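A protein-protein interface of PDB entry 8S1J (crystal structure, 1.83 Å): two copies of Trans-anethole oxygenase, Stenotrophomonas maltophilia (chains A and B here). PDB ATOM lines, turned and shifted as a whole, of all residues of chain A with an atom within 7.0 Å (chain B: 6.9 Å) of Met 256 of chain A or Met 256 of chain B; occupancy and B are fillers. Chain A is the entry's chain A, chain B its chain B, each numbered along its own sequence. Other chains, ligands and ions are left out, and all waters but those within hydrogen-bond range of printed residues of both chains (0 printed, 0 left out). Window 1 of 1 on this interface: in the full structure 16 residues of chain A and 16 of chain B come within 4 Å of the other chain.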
ATOM      1  N   ALA A 141     -17.192  19.568   9.972  1.00  0.00           N
ATOM      2  CA  ALA A 141     -16.872  19.066  11.294  1.00  0.00           C
ATOM      3  C   ALA A 141     -18.112  18.816  12.154  1.00  0.00           C
ATOM      4  O   ALA A 141     -17.978  18.460  13.324  1.00  0.00           O
ATOM      5  CB  ALA A 141     -15.916  20.026  11.981  1.00  0.00           C
ATOM      6  N   LEU A 223      -1.350  12.060  11.020  1.00  0.00           N
ATOM      7  CA  LEU A 223      -2.503  12.717  11.629  1.00  0.00           C
ATOM      8  C   LEU A 223      -2.904  13.974  10.854  1.00  0.00           C
ATOM      9  O   LEU A 223      -4.073  14.199  10.543  1.00  0.00           O
ATOM     10  CB  LEU A 223      -2.064  13.009  13.059  1.00  0.00           C
ATOM     11  CG  LEU A 223      -3.023  13.748  13.991  1.00  0.00           C
ATOM     12  CD1 LEU A 223      -4.484  13.389  13.851  1.00  0.00           C
ATOM     13  CD2 LEU A 223      -2.543  13.395  15.409  1.00  0.00           C
ATOM     14  N   GLN A 250     -11.213   9.798   9.792  1.00  0.00           N
ATOM     15  CA  GLN A 250     -11.934  10.996   9.404  1.00  0.00           C
ATOM     16  C   GLN A 250     -12.969  11.353  10.458  1.00  0.00           C
ATOM     17  O   GLN A 250     -13.115  12.508  10.833  1.00  0.00           O
ATOM     18  CB  GLN A 250     -12.622  10.774   8.057  1.00  0.00           C
ATOM     19  CG  GLN A 250     -13.572  11.896   7.649  1.00  0.00           C
ATOM     20  CD  GLN A 250     -14.122  11.734   6.245  1.00  0.00           C
ATOM     21  OE1 GLN A 250     -14.503  10.641   5.822  1.00  0.00           O
ATOM     22  NE2 GLN A 250     -14.157  12.820   5.490  1.00  0.00           N
ATOM     23  N   LYS A 251     -13.735  10.359  10.900  1.00  0.00           N
ATOM     24  CA  LYS A 251     -14.746  10.612  11.903  1.00  0.00           C
ATOM     25  C   LYS A 251     -14.071  11.115  13.178  1.00  0.00           C
ATOM     26  O   LYS A 251     -14.572  12.021  13.836  1.00  0.00           O
ATOM     27  CB  LYS A 251     -15.619   9.384  12.180  1.00  0.00           C
ATOM     28  CG  LYS A 251     -16.370   8.870  10.952  1.00  0.00           C
ATOM     29  CD  LYS A 251     -17.388   7.772  11.246  1.00  0.00           C
ATOM     30  CE  LYS A 251     -18.171   7.354  10.025  1.00  0.00           C
ATOM     31  NZ  LYS A 251     -19.202   6.363  10.343  1.00  0.00           N
ATOM     32  N   ILE A 252     -12.932  10.530  13.540  1.00  0.00           N
ATOM     33  CA  ILE A 252     -12.275  10.941  14.769  1.00  0.00           C
ATOM     34  C   ILE A 252     -11.692  12.349  14.613  1.00  0.00           C
ATOM     35  O   ILE A 252     -11.839  13.146  15.517  1.00  0.00           O
ATOM     36  CB  ILE A 252     -11.217   9.918  15.215  1.00  0.00           C
ATOM     37  CG1 ILE A 252     -11.876   8.603  15.662  1.00  0.00           C
ATOM     38  CG2 ILE A 252     -10.336  10.499  16.313  1.00  0.00           C
ATOM     39  CD1 ILE A 252     -10.917   7.414  15.749  1.00  0.00           C
ATOM     40  N   VAL A 253     -11.024  12.670  13.497  1.00  0.00           N
ATOM     41  CA  VAL A 253     -10.340  13.955  13.426  1.00  0.00           C
ATOM     42  C   VAL A 253     -11.380  15.079  13.328  1.00  0.00           C
ATOM     43  O   VAL A 253     -11.184  16.167  13.865  1.00  0.00           O
ATOM     44  CB  VAL A 253      -9.256  14.085  12.340  1.00  0.00           C
ATOM     45  CG1 VAL A 253      -8.181  13.019  12.512  1.00  0.00           C
ATOM     46  CG2 VAL A 253      -9.809  14.028  10.931  1.00  0.00           C
ATOM     47  N   LEU A 254     -12.503  14.812  12.662  1.00  0.00           N
ATOM     48  CA  LEU A 254     -13.557  15.800  12.544  1.00  0.00           C
ATOM     49  C   LEU A 254     -14.196  16.052  13.903  1.00  0.00           C
ATOM     50  O   LEU A 254     -14.546  17.196  14.200  1.00  0.00           O
ATOM     51  CB  LEU A 254     -14.585  15.457  11.474  1.00  0.00           C
ATOM     52  CG  LEU A 254     -14.052  15.457  10.034  1.00  0.00           C
ATOM     53  CD1 LEU A 254     -15.169  14.950   9.127  1.00  0.00           C
ATOM     54  CD2 LEU A 254     -13.535  16.835   9.637  1.00  0.00           C
ATOM     55  N   MET A 255     -14.319  15.012  14.726  1.00  0.00           N
ATOM     56  CA  MET A 255     -14.891  15.196  16.052  1.00  0.00           C
ATOM     57  C   MET A 255     -13.910  15.976  16.928  1.00  0.00           C
ATOM     58  O   MET A 255     -14.312  16.820  17.732  1.00  0.00           O
ATOM     59  CB  MET A 255     -15.282  13.866  16.709  1.00  0.00           C
ATOM     60  CG  MET A 255     -15.991  14.023  18.071  1.00  0.00           C
ATOM     61  SD  MET A 255     -17.495  15.033  18.080  1.00  0.00           S
ATOM     62  CE  MET A 255     -18.684  13.995  17.210  1.00  0.00           C
ATOM     63  N   MET A 256     -12.613  15.696  16.773  1.00  0.00           N
ATOM     64  CA  MET A 256     -11.633  16.411  17.571  1.00  0.00           C
ATOM     65  C   MET A 256     -11.646  17.895  17.212  1.00  0.00           C
ATOM     66  O   MET A 256     -11.515  18.714  18.098  1.00  0.00           O
ATOM     67  CB  MET A 256     -10.224  15.844  17.405  1.00  0.00           C
ATOM     68  CG  MET A 256     -10.069  14.456  18.042  1.00  0.00           C
ATOM     69  SD  MET A 256      -8.443  13.731  17.721  1.00  0.00           S
ATOM     70  CE  MET A 256      -7.498  14.791  18.823  1.00  0.00           C
ATOM     71  N   LEU A 257     -11.815  18.226  15.923  1.00  0.00           N
ATOM     72  CA  LEU A 257     -11.864  19.609  15.471  1.00  0.00           C
ATOM     73  C   LEU A 257     -13.133  20.279  15.984  1.00  0.00           C
ATOM     74  O   LEU A 257     -13.076  21.367  16.510  1.00  0.00           O
ATOM     75  CB  LEU A 257     -11.772  19.662  13.946  1.00  0.00           C
ATOM     76  CG  LEU A 257     -11.980  21.034  13.298  1.00  0.00           C
ATOM     77  CD1 LEU A 257     -10.909  22.003  13.672  1.00  0.00           C
ATOM     78  CD2 LEU A 257     -12.011  20.894  11.803  1.00  0.00           C
ATOM     79  N   ASN A 258     -14.268  19.587  15.846  1.00  0.00           N
ATOM     80  CA  ASN A 258     -15.531  19.982  16.441  1.00  0.00           C
ATOM     81  C   ASN A 258     -15.331  20.335  17.914  1.00  0.00           C
ATOM     82  O   ASN A 258     -15.724  21.419  18.345  1.00  0.00           O
ATOM     83  CB  ASN A 258     -16.558  18.868  16.256  1.00  0.00           C
ATOM     84  CG  ASN A 258     -17.907  19.178  16.865  1.00  0.00           C
ATOM     85  OD1 ASN A 258     -18.016  19.572  18.045  1.00  0.00           O
ATOM     86  ND2 ASN A 258     -18.955  18.961  16.083  1.00  0.00           N
ATOM     87  N   GLN A 259     -14.745  19.420  18.699  1.00  0.00           N
ATOM     88  CA  GLN A 259     -14.596  19.627  20.146  1.00  0.00           C
ATOM     89  C   GLN A 259     -13.666  20.797  20.481  1.00  0.00           C
ATOM     90  O   GLN A 259     -13.913  21.534  21.428  1.00  0.00           O
ATOM     91  CB  GLN A 259     -14.133  18.339  20.831  1.00  0.00           C
ATOM     92  CG  GLN A 259     -15.252  17.296  20.892  1.00  0.00           C
ATOM     93  CD  GLN A 259     -14.815  15.921  21.344  1.00  0.00           C
ATOM     94  OE1 GLN A 259     -15.379  15.335  22.280  1.00  0.00           O
ATOM     95  NE2 GLN A 259     -13.817  15.375  20.661  1.00  0.00           N
ATOM     96  N   TYR A 260     -12.573  20.953  19.739  1.00  0.00           N
ATOM     97  CA  TYR A 260     -11.657  22.056  19.978  1.00  0.00           C
ATOM     98  C   TYR A 260     -12.380  23.383  19.758  1.00  0.00           C
ATOM     99  O   TYR A 260     -12.277  24.286  20.583  1.00  0.00           O
ATOM    100  CB  TYR A 260     -10.440  21.948  19.069  1.00  0.00           C
ATOM    101  CG  TYR A 260      -9.597  23.216  18.985  1.00  0.00           C
ATOM    102  CD1 TYR A 260      -8.795  23.628  20.039  1.00  0.00           C
ATOM    103  CD2 TYR A 260      -9.553  23.963  17.821  1.00  0.00           C
ATOM    104  CE1 TYR A 260      -8.022  24.774  19.951  1.00  0.00           C
ATOM    105  CE2 TYR A 260      -8.784  25.115  17.721  1.00  0.00           C
ATOM    106  CZ  TYR A 260      -8.009  25.526  18.790  1.00  0.00           C
ATOM    107  OH  TYR A 260      -7.241  26.654  18.669  1.00  0.00           O
ATOM    108  N   LEU A 261     -13.119  23.500  18.646  1.00  0.00           N
ATOM    109  CA  LEU A 261     -13.835  24.741  18.363  1.00  0.00           C
ATOM    110  C   LEU A 261     -14.927  24.960  19.402  1.00  0.00           C
ATOM    111  O   LEU A 261     -15.112  26.084  19.845  1.00  0.00           O
ATOM    112  CB  LEU A 261     -14.346  24.794  16.923  1.00  0.00           C
ATOM    113  CG  LEU A 261     -13.236  24.974  15.893  1.00  0.00           C
ATOM    114  CD1 LEU A 261     -13.715  24.883  14.452  1.00  0.00           C
ATOM    115  CD2 LEU A 261     -12.523  26.298  16.139  1.00  0.00           C
ATOM    116  N   THR A 262     -15.611  23.892  19.824  1.00  0.00           N
ATOM    117  CA  THR A 262     -16.613  24.037  20.868  1.00  0.00           C
ATOM    118  C   THR A 262     -15.970  24.577  22.143  1.00  0.00           C
ATOM    119  O   THR A 262     -16.507  25.450  22.803  1.00  0.00           O
ATOM    120  CB  THR A 262     -17.340  22.715  21.119  1.00  0.00           C
ATOM    121  OG1 THR A 262     -17.929  22.380  19.876  1.00  0.00           O
ATOM    122  CG2 THR A 262     -18.466  22.880  22.123  1.00  0.00           C
ATOM    123  N   LEU A 263     -14.805  24.050  22.492  1.00  0.00           N
ATOM    124  CA  LEU A 263     -14.157  24.401  23.742  1.00  0.00           C
ATOM    125  C   LEU A 263     -13.806  25.885  23.734  1.00  0.00           C
ATOM    126  O   LEU A 263     -14.091  26.613  24.693  1.00  0.00           O
ATOM    127  CB  LEU A 263     -12.927  23.505  23.843  1.00  0.00           C
ATOM    128  CG  LEU A 263     -12.265  23.333  25.207  1.00  0.00           C
ATOM    129  CD1 LEU A 263     -13.138  22.824  26.344  1.00  0.00           C
ATOM    130  CD2 LEU A 263     -11.165  22.320  24.956  1.00  0.00           C
ATOM    131  N   LEU B 223      -6.536  26.408  27.426  1.00  0.00           N
ATOM    132  CA  LEU B 223      -6.748  25.026  27.022  1.00  0.00           C
ATOM    133  C   LEU B 223      -5.732  24.100  27.697  1.00  0.00           C
ATOM    134  O   LEU B 223      -6.073  23.027  28.203  1.00  0.00           O
ATOM    135  CB  LEU B 223      -6.631  25.014  25.496  1.00  0.00           C
ATOM    136  CG  LEU B 223      -6.735  23.656  24.793  1.00  0.00           C
ATOM    137  CD1 LEU B 223      -7.859  22.784  25.294  1.00  0.00           C
ATOM    138  CD2 LEU B 223      -6.923  23.868  23.320  1.00  0.00           C
ATOM    139  N   GLN B 250     -13.263  19.717  31.117  1.00  0.00           N
ATOM    140  CA  GLN B 250     -12.606  18.488  31.521  1.00  0.00           C
ATOM    141  C   GLN B 250     -13.124  17.316  30.698  1.00  0.00           C
ATOM    142  O   GLN B 250     -12.357  16.474  30.250  1.00  0.00           O
ATOM    143  CB  GLN B 250     -12.873  18.217  33.005  1.00  0.00           C
ATOM    144  CG  GLN B 250     -12.351  16.864  33.482  1.00  0.00           C
ATOM    145  CD  GLN B 250     -12.464  16.686  34.982  1.00  0.00           C
ATOM    146  OE1 GLN B 250     -13.454  17.088  35.608  1.00  0.00           O
ATOM    147  NE2 GLN B 250     -11.422  16.114  35.566  1.00  0.00           N
ATOM    148  N   LYS B 251     -14.450  17.217  30.579  1.00  0.00           N
ATOM    149  CA  LYS B 251     -15.022  16.122  29.826  1.00  0.00           C
ATOM    150  C   LYS B 251     -14.567  16.225  28.368  1.00  0.00           C
ATOM    151  O   LYS B 251     -14.286  15.220  27.725  1.00  0.00           O
ATOM    152  CB  LYS B 251     -16.544  16.110  29.954  1.00  0.00           C
ATOM    153  CG  LYS B 251     -17.078  15.777  31.334  1.00  0.00           C
ATOM    154  CD  LYS B 251     -18.505  15.212  31.313  1.00  0.00           C
ATOM    155  CE  LYS B 251     -19.247  15.251  32.622  1.00  0.00           C
ATOM    156  NZ  LYS B 251     -19.690  16.612  32.948  1.00  0.00           N
ATOM    157  N   ILE B 252     -14.491  17.445  27.834  1.00  0.00           N
ATOM    158  CA  ILE B 252     -14.082  17.596  26.451  1.00  0.00           C
ATOM    159  C   ILE B 252     -12.600  17.247  26.286  1.00  0.00           C
ATOM    160  O   ILE B 252     -12.248  16.555  25.341  1.00  0.00           O
ATOM    161  CB  ILE B 252     -14.417  18.996  25.919  1.00  0.00           C
ATOM    162  CG1 ILE B 252     -15.940  19.186  25.822  1.00  0.00           C
ATOM    163  CG2 ILE B 252     -13.708  19.232  24.592  1.00  0.00           C
ATOM    164  CD1 ILE B 252     -16.381  20.621  25.582  1.00  0.00           C
ATOM    165  N   VAL B 253     -11.724  17.726  27.168  1.00  0.00           N
ATOM    166  CA  VAL B 253     -10.306  17.548  26.916  1.00  0.00           C
ATOM    167  C   VAL B 253      -9.952  16.070  27.114  1.00  0.00           C
ATOM    168  O   VAL B 253      -9.100  15.537  26.412  1.00  0.00           O
ATOM    169  CB  VAL B 253      -9.357  18.489  27.694  1.00  0.00           C
ATOM    170  CG1 VAL B 253      -9.653  19.941  27.375  1.00  0.00           C
ATOM    171  CG2 VAL B 253      -9.365  18.277  29.183  1.00  0.00           C
ATOM    172  N   LEU B 254     -10.640  15.401  28.038  1.00  0.00           N
ATOM    173  CA  LEU B 254     -10.391  13.991  28.277  1.00  0.00           C
ATOM    174  C   LEU B 254     -10.854  13.164  27.083  1.00  0.00           C
ATOM    175  O   LEU B 254     -10.207  12.178  26.757  1.00  0.00           O
ATOM    176  CB  LEU B 254     -10.998  13.514  29.596  1.00  0.00           C
ATOM    177  CG  LEU B 254     -10.327  14.088  30.850  1.00  0.00           C
ATOM    178  CD1 LEU B 254     -11.027  13.643  32.100  1.00  0.00           C
ATOM    179  CD2 LEU B 254      -8.852  13.747  30.935  1.00  0.00           C
ATOM    180  N   MET B 255     -11.967  13.543  26.444  1.00  0.00           N
ATOM    181  CA  MET B 255     -12.420  12.827  25.260  1.00  0.00           C
ATOM    182  C   MET B 255     -11.444  13.073  24.109  1.00  0.00           C
ATOM    183  O   MET B 255     -11.138  12.147  23.344  1.00  0.00           O
ATOM    184  CB  MET B 255     -13.849  13.218  24.866  1.00  0.00           C
ATOM    185  CG  MET B 255     -14.418  12.453  23.665  1.00  0.00           C
ATOM    186  SD  MET B 255     -14.452  10.644  23.745  1.00  0.00           S
ATOM    187  CE  MET B 255     -15.504  10.343  22.313  1.00  0.00           C
ATOM    188  N   MET B 256     -10.925  14.307  24.001  1.00  0.00           N
ATOM    189  CA  MET B 256      -9.984  14.600  22.926  1.00  0.00           C
ATOM    190  C   MET B 256      -8.725  13.749  23.098  1.00  0.00           C
ATOM    191  O   MET B 256      -8.181  13.295  22.117  1.00  0.00           O
ATOM    192  CB  MET B 256      -9.605  16.085  22.837  1.00  0.00           C
ATOM    193  CG  MET B 256     -10.734  16.962  22.345  1.00  0.00           C
ATOM    194  SD  MET B 256     -10.381  18.732  22.390  1.00  0.00           S
ATOM    195  CE  MET B 256      -8.967  18.978  21.318  1.00  0.00           C
ATOM    196  N   LEU B 257      -8.267  13.550  24.344  1.00  0.00           N
ATOM    197  CA  LEU B 257      -7.072  12.780  24.635  1.00  0.00           C
ATOM    198  C   LEU B 257      -7.331  11.306  24.352  1.00  0.00           C
ATOM    199  O   LEU B 257      -6.536  10.687  23.674  1.00  0.00           O
ATOM    200  CB  LEU B 257      -6.630  13.010  26.078  1.00  0.00           C
ATOM    201  CG  LEU B 257      -5.466  12.148  26.587  1.00  0.00           C
ATOM    202  CD1 LEU B 257      -4.198  12.446  25.869  1.00  0.00           C
ATOM    203  CD2 LEU B 257      -5.275  12.391  28.074  1.00  0.00           C
ATOM    204  N   ASN B 258      -8.473  10.791  24.838  1.00  0.00           N
ATOM    205  CA  ASN B 258      -8.979   9.475  24.477  1.00  0.00           C
ATOM    206  C   ASN B 258      -8.900   9.268  22.953  1.00  0.00           C
ATOM    207  O   ASN B 258      -8.316   8.291  22.482  1.00  0.00           O
ATOM    208  CB  ASN B 258     -10.402   9.304  24.996  1.00  0.00           C
ATOM    209  CG  ASN B 258     -11.025   7.958  24.667  1.00  0.00           C
ATOM    210  OD1 ASN B 258     -11.016   7.513  23.508  1.00  0.00           O
ATOM    211  ND2 ASN B 258     -11.604   7.311  25.671  1.00  0.00           N
ATOM    212  N   GLN B 259      -9.487  10.181  22.178  1.00  0.00           N
ATOM    213  CA  GLN B 259      -9.578  10.026  20.729  1.00  0.00           C
ATOM    214  C   GLN B 259      -8.206  10.070  20.044  1.00  0.00           C
ATOM    215  O   GLN B 259      -7.954   9.332  19.092  1.00  0.00           O
ATOM    216  CB  GLN B 259     -10.507  11.083  20.126  1.00  0.00           C
ATOM    217  CG  GLN B 259     -11.977  10.867  20.433  1.00  0.00           C
ATOM    218  CD  GLN B 259     -12.817  12.066  20.047  1.00  0.00           C
ATOM    219  OE1 GLN B 259     -12.623  13.178  20.555  1.00  0.00           O
ATOM    220  NE2 GLN B 259     -13.748  11.854  19.130  1.00  0.00           N
ATOM    221  N   TYR B 260      -7.334  10.969  20.477  1.00  0.00           N
ATOM    222  CA  TYR B 260      -5.995  11.046  19.914  1.00  0.00           C
ATOM    223  C   TYR B 260      -5.236   9.738  20.133  1.00  0.00           C
ATOM    224  O   TYR B 260      -4.625   9.209  19.206  1.00  0.00           O
ATOM    225  CB  TYR B 260      -5.250  12.194  20.570  1.00  0.00           C
ATOM    226  CG  TYR B 260      -3.755  12.238  20.322  1.00  0.00           C
ATOM    227  CD1 TYR B 260      -3.244  12.617  19.094  1.00  0.00           C
ATOM    228  CD2 TYR B 260      -2.855  11.965  21.338  1.00  0.00           C
ATOM    229  CE1 TYR B 260      -1.880  12.729  18.884  1.00  0.00           C
ATOM    230  CE2 TYR B 260      -1.486  12.055  21.135  1.00  0.00           C
ATOM    231  CZ  TYR B 260      -0.990  12.420  19.896  1.00  0.00           C
ATOM    232  OH  TYR B 260       0.370  12.508  19.707  1.00  0.00           O
ATOM    233  N   LEU B 261      -5.297   9.194  21.354  1.00  0.00           N
ATOM    234  CA  LEU B 261      -4.614   7.937  21.634  1.00  0.00           C
ATOM    235  C   LEU B 261      -5.265   6.802  20.855  1.00  0.00           C
ATOM    236  O   LEU B 261      -4.556   5.947  20.319  1.00  0.00           O
ATOM    237  CB  LEU B 261      -4.535   7.675  23.135  1.00  0.00           C
ATOM    238  CG  LEU B 261      -3.569   8.593  23.890  1.00  0.00           C
ATOM    239  CD1 LEU B 261      -3.613   8.404  25.374  1.00  0.00           C
ATOM    240  CD2 LEU B 261      -2.171   8.430  23.384  1.00  0.00           C
ATOM    241  N   THR B 262      -6.598   6.810  20.726  1.00  0.00           N
ATOM    242  CA  THR B 262      -7.263   5.783  19.937  1.00  0.00           C
ATOM    243  C   THR B 262      -6.750   5.853  18.499  1.00  0.00           C
ATOM    244  O   THR B 262      -6.444   4.845  17.889  1.00  0.00           O
ATOM    245  CB  THR B 262      -8.782   5.959  20.025  1.00  0.00           C
ATOM    246  OG1 THR B 262      -9.091   5.728  21.394  1.00  0.00           O
ATOM    247  CG2 THR B 262      -9.568   4.968  19.202  1.00  0.00           C
ATOM    248  N   LEU B 263      -6.641   7.067  17.962  1.00  0.00           N
ATOM    249  CA  LEU B 263      -6.276   7.242  16.571  1.00  0.00           C
ATOM    250  C   LEU B 263      -4.882   6.672  16.307  1.00  0.00           C
ATOM    251  O   LEU B 263      -4.665   5.952  15.327  1.00  0.00           O
ATOM    252  CB  LEU B 263      -6.372   8.738  16.283  1.00  0.00           C
ATOM    253  CG  LEU B 263      -6.408   9.151  14.811  1.00  0.00           C
ATOM    254  CD1 LEU B 263      -7.674   8.715  14.111  1.00  0.00           C
ATOM    255  CD2 LEU B 263      -6.226  10.653  14.797  1.00  0.00           C
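CE1 of Tyr 260 of chain B touches CD2 of Leu 223 of chain A (3.6 Å).
Leu 223 of chain A touches Leu 263 of chain B (CD1 to CD2, 3.4 Å).
Ile 252 of chain A touches Gln 259 of chain B.
CG1 of Val 253 of chain A touches CD2 of Leu 263 of chain B (3.8 Å).
CG of Met 255 of chain A touches NE2 of Gln 259 of chain B, 3.3 Å away.
Met 256 of chain A touches Gln 259 of chain B.
Gln 259 of chain A touches Met 256 of chain B.
Tyr 260 of chain A touches Leu 223 of chain B.
CD2 of Leu 263 of chain A touches CD1 of Leu 223 of chain B (3.4 Å).
Ile 252 of chain B touches Leu 263 of chain A.
Leu 223 of chain A touches Tyr 260 of chain B, and with the chains exchanged Tyr 260 of chain A touches Leu 223 of chain B.
Leu 223 of chain A touches Leu 263 of chain B, and with the chains exchanged Leu 263 of chain A touches Leu 223 of chain B.
Ile 252 of chain A touches Leu 263 of chain B, and with the chains exchanged Leu 263 of chain A touches Ile 252 of chain B.
Gln 259 of chain A touches its own counterpart, Gln 259 of chain B.
Positions printed for both chains: 223, 250, 251, 252, 253, 254, 255, 256, 257, 258, 259, 260, 261, 262 and 263.
Of the 17 pairs that touch across the chains among the printed residues, 16 have their exchanged pair printed and touching as well.
The backbone carbonyl oxygen (O) of Met 255 of chain A sits at hydrogen-bond distance from the side-chain amide nitrogen (NE2) of Gln 259 of chain A.
The backbone carbonyl oxygen of Met 255 of chain B lies close to the side-chain amide oxygen of Gln 259 of chain B, 3.3 Å away.
The side-chain amide oxygen (OE1) of Gln 259 of chain B sits at hydrogen-bond distance from the side-chain amide nitrogen (NE2) of Gln 259 of chain A.
Hydrophobic or aromatic side chains of chain A that line the printed part of chain B: Leu 223, Ile 252, Val 253, Met 255, Met 256, Tyr 260 and Leu 263.
Of the printed residues of chain B, Met 256 of chain A touches Met 256, Gln 259 and Tyr 260.
Of the printed residues of chain A, Met 256 of chain B touches Met 256 and Gln 259.
Of the printed residues of chain B, Val 253 of chain A touches Leu 263.
Of the printed residues of chain A, Gln 259 of chain B touches Ile 252 (3.8 Å), Met 255 (3.3 Å), Met 256 (3.8 Å) and Gln 259 (2.5 Å).
Of the printed residues of chain B, Tyr 260 of chain A touches Leu 223 (3.7 Å).
Printed residues of chain A within 4 Å of Met 255 of chain B: Gln 259 (3.3 Å).
Lys 251 of chain B touches none of the printed residues of chain A.
Gln 250 of chain B touches none of the printed residues of chain A.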
